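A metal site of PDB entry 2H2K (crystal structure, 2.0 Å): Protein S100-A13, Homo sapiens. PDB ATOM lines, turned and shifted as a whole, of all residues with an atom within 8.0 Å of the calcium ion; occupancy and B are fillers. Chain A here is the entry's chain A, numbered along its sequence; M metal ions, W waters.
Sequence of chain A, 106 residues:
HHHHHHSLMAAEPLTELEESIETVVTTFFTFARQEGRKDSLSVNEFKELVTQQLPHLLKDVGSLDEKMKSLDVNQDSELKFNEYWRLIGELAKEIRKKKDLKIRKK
The side-chain carboxylate (OD1) of Asp 72 sits close to the backbone NH (N) of Gln 75, at 3.4 Å.
The side-chain carboxylate of Asp 72 sits at hydrogen-bond distance from the backbone NH of Ser 77, at 2.7 Å.
The side-chain carboxylate (OE1) of Glu 83 sits close to the backbone NH (N) of Lys 80 (3.0 Å).
OE2 of Glu 83 sits close to N of Val 73, at 3.1 Å.
Water W1 lies within hydrogen-bond range of the side-chain carboxylate (OD2) of Asp 76 (3.1 Å), the backbone NH (N) of Lys 80 (3.5 Å) and the side-chain amide nitrogen (ND2) of Asn 74 (3.5 Å).
The calcium ion is bound by OD1 of Asp 72 (2.3 Å).
O of Glu 78 is bound to the calcium ion (2.3 Å).
The calcium ion is bound by the side-chain amide oxygen (OD1) of Asn 74, 2.4 Å away.
The calcium ion is bound by OE1 of Glu 83, 2.4 Å away.
The calcium ion is bound by water W1, at 2.4 Å.
The calcium ion is bound by OD1 of Asp 76 (2.4 Å).
The calcium ion is bound by the side-chain carboxylate (OE2) of Glu 83, at 2.5 Å.
The calcium ion has seven donor atoms within binding distance.
Five residues have an atom within 4 Å of the calcium ion: Asp 72, Asn 74, Asp 76, Glu 78 and Glu 83.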
ATOM      1  N   SER A  40     -32.043 -16.827 -25.120  1.00  0.00           N
ATOM      2  CA  SER A  40     -30.709 -16.669 -25.682  1.00  0.00           C
ATOM      3  C   SER A  40     -29.765 -17.743 -25.172  1.00  0.00           C
ATOM      4  O   SER A  40     -29.883 -18.191 -24.038  1.00  0.00           O
ATOM      5  CB  SER A  40     -30.154 -15.278 -25.364  1.00  0.00           C
ATOM      6  OG  SER A  40     -29.653 -15.230 -24.036  1.00  0.00           O
ATOM      7  N   LEU A  41     -28.828 -18.159 -26.018  1.00  0.00           N
ATOM      8  CA  LEU A  41     -27.775 -19.084 -25.609  1.00  0.00           C
ATOM      9  C   LEU A  41     -26.596 -18.333 -24.995  1.00  0.00           C
ATOM     10  O   LEU A  41     -25.935 -17.536 -25.673  1.00  0.00           O
ATOM     11  CB  LEU A  41     -27.312 -19.917 -26.798  1.00  0.00           C
ATOM     12  CG  LEU A  41     -28.401 -20.646 -27.593  1.00  0.00           C
ATOM     13  CD1 LEU A  41     -27.921 -20.965 -28.997  1.00  0.00           C
ATOM     14  CD2 LEU A  41     -28.845 -21.906 -26.871  1.00  0.00           C
ATOM     15  N   MET A  68     -18.370 -18.783 -31.060  1.00  0.00           N
ATOM     16  CA  MET A  68     -19.297 -17.979 -30.287  1.00  0.00           C
ATOM     17  C   MET A  68     -19.142 -16.489 -30.606  1.00  0.00           C
ATOM     18  O   MET A  68     -20.124 -15.806 -30.873  1.00  0.00           O
ATOM     19  CB  MET A  68     -19.083 -18.216 -28.783  1.00  0.00           C
ATOM     20  CG  MET A  68     -19.998 -17.390 -27.888  1.00  0.00           C
ATOM     21  SD  MET A  68     -21.684 -18.016 -27.873  1.00  0.00           S
ATOM     22  CE  MET A  68     -22.377 -17.093 -26.494  1.00  0.00           C
ATOM     23  N   LYS A  69     -17.903 -16.016 -30.584  1.00  0.00           N
ATOM     24  CA  LYS A  69     -17.629 -14.593 -30.790  1.00  0.00           C
ATOM     25  C   LYS A  69     -18.088 -14.141 -32.174  1.00  0.00           C
ATOM     26  O   LYS A  69     -18.723 -13.097 -32.312  1.00  0.00           O
ATOM     27  CB  LYS A  69     -16.134 -14.310 -30.615  1.00  0.00           C
ATOM     28  CG  LYS A  69     -15.701 -14.123 -29.176  1.00  0.00           C
ATOM     29  CD  LYS A  69     -14.190 -14.019 -29.063  1.00  0.00           C
ATOM     30  CE  LYS A  69     -13.715 -14.398 -27.664  1.00  0.00           C
ATOM     31  NZ  LYS A  69     -12.240 -14.582 -27.622  1.00  0.00           N
ATOM     32  N   LEU A  71     -20.385 -15.463 -34.043  1.00  0.00           N
ATOM     33  CA  LEU A  71     -21.845 -15.529 -34.163  1.00  0.00           C
ATOM     34  C   LEU A  71     -22.556 -14.438 -33.353  1.00  0.00           C
ATOM     35  O   LEU A  71     -23.674 -14.048 -33.678  1.00  0.00           O
ATOM     36  CB  LEU A  71     -22.350 -16.901 -33.719  1.00  0.00           C
ATOM     37  CG  LEU A  71     -21.985 -18.074 -34.629  1.00  0.00           C
ATOM     38  CD1 LEU A  71     -22.326 -19.391 -33.954  1.00  0.00           C
ATOM     39  CD2 LEU A  71     -22.711 -17.939 -35.951  1.00  0.00           C
ATOM     40  N   ASP A  72     -21.895 -13.960 -32.308  1.00  0.00           N
ATOM     41  CA  ASP A  72     -22.431 -12.923 -31.425  1.00  0.00           C
ATOM     42  C   ASP A  72     -22.187 -11.586 -32.108  1.00  0.00           C
ATOM     43  O   ASP A  72     -21.371 -10.779 -31.654  1.00  0.00           O
ATOM     44  CB  ASP A  72     -21.697 -12.979 -30.078  1.00  0.00           C
ATOM     45  CG  ASP A  72     -22.246 -11.990 -29.067  1.00  0.00           C
ATOM     46  OD1 ASP A  72     -23.364 -11.472 -29.273  1.00  0.00           O
ATOM     47  OD2 ASP A  72     -21.558 -11.750 -28.049  1.00  0.00           O
ATOM     48  N   VAL A  73     -22.903 -11.336 -33.201  1.00  0.00           N
ATOM     49  CA  VAL A  73     -22.702 -10.122 -33.972  1.00  0.00           C
ATOM     50  C   VAL A  73     -23.026  -8.783 -33.282  1.00  0.00           C
ATOM     51  O   VAL A  73     -22.616  -7.733 -33.767  1.00  0.00           O
ATOM     52  CB  VAL A  73     -23.438 -10.223 -35.340  1.00  0.00           C
ATOM     53  CG1 VAL A  73     -22.853 -11.372 -36.142  1.00  0.00           C
ATOM     54  CG2 VAL A  73     -24.921 -10.439 -35.130  1.00  0.00           C
ATOM     55  N   ASN A  74     -23.742  -8.808 -32.168  1.00  0.00           N
ATOM     56  CA  ASN A  74     -24.048  -7.568 -31.455  1.00  0.00           C
ATOM     57  C   ASN A  74     -23.246  -7.523 -30.152  1.00  0.00           C
ATOM     58  O   ASN A  74     -23.532  -6.724 -29.259  1.00  0.00           O
ATOM     59  CB  ASN A  74     -25.553  -7.455 -31.171  1.00  0.00           C
ATOM     60  CG  ASN A  74     -26.004  -8.378 -30.055  1.00  0.00           C
ATOM     61  OD1 ASN A  74     -25.303  -9.298 -29.670  1.00  0.00           O
ATOM     62  ND2 ASN A  74     -27.207  -8.135 -29.547  1.00  0.00           N
ATOM     63  N   GLN A  75     -22.247  -8.391 -30.079  1.00  0.00           N
ATOM     64  CA  GLN A  75     -21.352  -8.513 -28.920  1.00  0.00           C
ATOM     65  C   GLN A  75     -22.014  -8.346 -27.563  1.00  0.00           C
ATOM     66  O   GLN A  75     -21.574  -7.514 -26.761  1.00  0.00           O
ATOM     67  CB  GLN A  75     -20.192  -7.512 -29.020  1.00  0.00           C
ATOM     68  CG  GLN A  75     -19.192  -7.760 -30.137  1.00  0.00           C
ATOM     69  CD  GLN A  75     -19.565  -7.055 -31.425  1.00  0.00           C
ATOM     70  OE1 GLN A  75     -20.076  -5.937 -31.408  1.00  0.00           O
ATOM     71  NE2 GLN A  75     -19.294  -7.696 -32.557  1.00  0.00           N
ATOM     72  N   ASP A  76     -23.056  -9.110 -27.268  1.00  0.00           N
ATOM     73  CA  ASP A  76     -23.701  -9.001 -25.967  1.00  0.00           C
ATOM     74  C   ASP A  76     -23.517 -10.279 -25.157  1.00  0.00           C
ATOM     75  O   ASP A  76     -24.178 -10.497 -24.138  1.00  0.00           O
ATOM     76  CB  ASP A  76     -25.189  -8.665 -26.129  1.00  0.00           C
ATOM     77  CG  ASP A  76     -26.004  -9.810 -26.686  1.00  0.00           C
ATOM     78  OD1 ASP A  76     -25.409 -10.843 -27.079  1.00  0.00           O
ATOM     79  OD2 ASP A  76     -27.248  -9.676 -26.756  1.00  0.00           O
ATOM     80  N   SER A  77     -22.591 -11.114 -25.611  1.00  0.00           N
ATOM     81  CA  SER A  77     -22.238 -12.381 -24.954  1.00  0.00           C
ATOM     82  C   SER A  77     -23.270 -13.501 -24.995  1.00  0.00           C
ATOM     83  O   SER A  77     -23.116 -14.529 -24.337  1.00  0.00           O
ATOM     84  CB  SER A  77     -21.863 -12.106 -23.487  1.00  0.00           C
ATOM     85  OG  SER A  77     -20.763 -11.207 -23.413  1.00  0.00           O
ATOM     86  N   GLU A  78     -24.326 -13.311 -25.776  1.00  0.00           N
ATOM     87  CA  GLU A  78     -25.379 -14.314 -25.888  1.00  0.00           C
ATOM     88  C   GLU A  78     -25.751 -14.481 -27.357  1.00  0.00           C
ATOM     89  O   GLU A  78     -25.509 -13.588 -28.171  1.00  0.00           O
ATOM     90  CB  GLU A  78     -26.633 -13.853 -25.143  1.00  0.00           C
ATOM     91  CG  GLU A  78     -26.463 -13.594 -23.644  1.00  0.00           C
ATOM     92  CD  GLU A  78     -26.598 -14.858 -22.818  1.00  0.00           C
ATOM     93  OE1 GLU A  78     -27.540 -15.636 -23.087  1.00  0.00           O
ATOM     94  OE2 GLU A  78     -25.783 -15.056 -21.903  1.00  0.00           O
ATOM     95  N   LEU A  79     -26.329 -15.622 -27.698  1.00  0.00           N
ATOM     96  CA  LEU A  79     -26.770 -15.844 -29.070  1.00  0.00           C
ATOM     97  C   LEU A  79     -28.294 -15.874 -29.036  1.00  0.00           C
ATOM     98  O   LEU A  79     -28.895 -16.816 -28.510  1.00  0.00           O
ATOM     99  CB  LEU A  79     -26.241 -17.164 -29.632  1.00  0.00           C
ATOM    100  CG  LEU A  79     -24.719 -17.373 -29.742  1.00  0.00           C
ATOM    101  CD1 LEU A  79     -24.459 -18.635 -30.567  1.00  0.00           C
ATOM    102  CD2 LEU A  79     -24.072 -16.160 -30.420  1.00  0.00           C
ATOM    103  N   LYS A  80     -28.924 -14.825 -29.544  1.00  0.00           N
ATOM    104  CA  LYS A  80     -30.373 -14.793 -29.587  1.00  0.00           C
ATOM    105  C   LYS A  80     -30.759 -15.613 -30.811  1.00  0.00           C
ATOM    106  O   LYS A  80     -29.884 -16.001 -31.595  1.00  0.00           O
ATOM    107  CB  LYS A  80     -30.889 -13.357 -29.689  1.00  0.00           C
ATOM    108  CG  LYS A  80     -31.680 -12.908 -28.461  1.00  0.00           C
ATOM    109  CD  LYS A  80     -32.228 -11.498 -28.584  1.00  0.00           C
ATOM    110  CE  LYS A  80     -31.176 -10.447 -28.248  1.00  0.00           C
ATOM    111  NZ  LYS A  80     -31.740  -9.065 -28.312  1.00  0.00           N
ATOM    112  N   PHE A  81     -32.040 -15.888 -30.989  1.00  0.00           N
ATOM    113  CA  PHE A  81     -32.471 -16.694 -32.121  1.00  0.00           C
ATOM    114  C   PHE A  81     -31.943 -16.265 -33.494  1.00  0.00           C
ATOM    115  O   PHE A  81     -31.519 -17.105 -34.281  1.00  0.00           O
ATOM    116  CB  PHE A  81     -33.995 -16.768 -32.191  1.00  0.00           C
ATOM    117  CG  PHE A  81     -34.484 -17.736 -33.213  1.00  0.00           C
ATOM    118  CD1 PHE A  81     -34.575 -19.097 -32.915  1.00  0.00           C
ATOM    119  CD2 PHE A  81     -34.800 -17.316 -34.502  1.00  0.00           C
ATOM    120  CE1 PHE A  81     -34.973 -20.009 -33.895  1.00  0.00           C
ATOM    121  CE2 PHE A  81     -35.192 -18.220 -35.480  1.00  0.00           C
ATOM    122  CZ  PHE A  81     -35.277 -19.574 -35.172  1.00  0.00           C
ATOM    123  N   GLU A  83     -29.209 -14.838 -34.292  1.00  0.00           N
ATOM    124  CA  GLU A  83     -27.791 -15.193 -34.431  1.00  0.00           C
ATOM    125  C   GLU A  83     -27.656 -16.711 -34.609  1.00  0.00           C
ATOM    126  O   GLU A  83     -26.802 -17.184 -35.349  1.00  0.00           O
ATOM    127  CB  GLU A  83     -27.010 -14.700 -33.207  1.00  0.00           C
ATOM    128  CG  GLU A  83     -27.002 -13.180 -33.101  1.00  0.00           C
ATOM    129  CD  GLU A  83     -26.395 -12.680 -31.803  1.00  0.00           C
ATOM    130  OE1 GLU A  83     -26.689 -13.268 -30.746  1.00  0.00           O
ATOM    131  OE2 GLU A  83     -25.634 -11.694 -31.857  1.00  0.00           O
ATOM    132  N   TYR A  84     -28.507 -17.450 -33.905  1.00  0.00           N
ATOM    133  CA  TYR A  84     -28.505 -18.903 -34.006  1.00  0.00           C
ATOM    134  C   TYR A  84     -28.940 -19.250 -35.427  1.00  0.00           C
ATOM    135  O   TYR A  84     -28.345 -20.120 -36.079  1.00  0.00           O
ATOM    136  CB  TYR A  84     -29.483 -19.486 -32.978  1.00  0.00           C
ATOM    137  CG  TYR A  84     -29.955 -20.902 -33.249  1.00  0.00           C
ATOM    138  CD1 TYR A  84     -29.149 -22.014 -32.949  1.00  0.00           C
ATOM    139  CD2 TYR A  84     -31.235 -21.147 -33.736  1.00  0.00           C
ATOM    140  CE1 TYR A  84     -29.617 -23.327 -33.133  1.00  0.00           C
ATOM    141  CE2 TYR A  84     -31.721 -22.435 -33.918  1.00  0.00           C
ATOM    142  CZ  TYR A  84     -30.912 -23.525 -33.607  1.00  0.00           C
ATOM    143  OH  TYR A  84     -31.423 -24.798 -33.757  1.00  0.00           O
HETATM  144 CA    CA M   1     -25.634 -11.630 -29.366  1.00  0.00          CA
HETATM  145  O   HOH W   1     -28.017 -11.497 -29.096  1.00  0.00           O
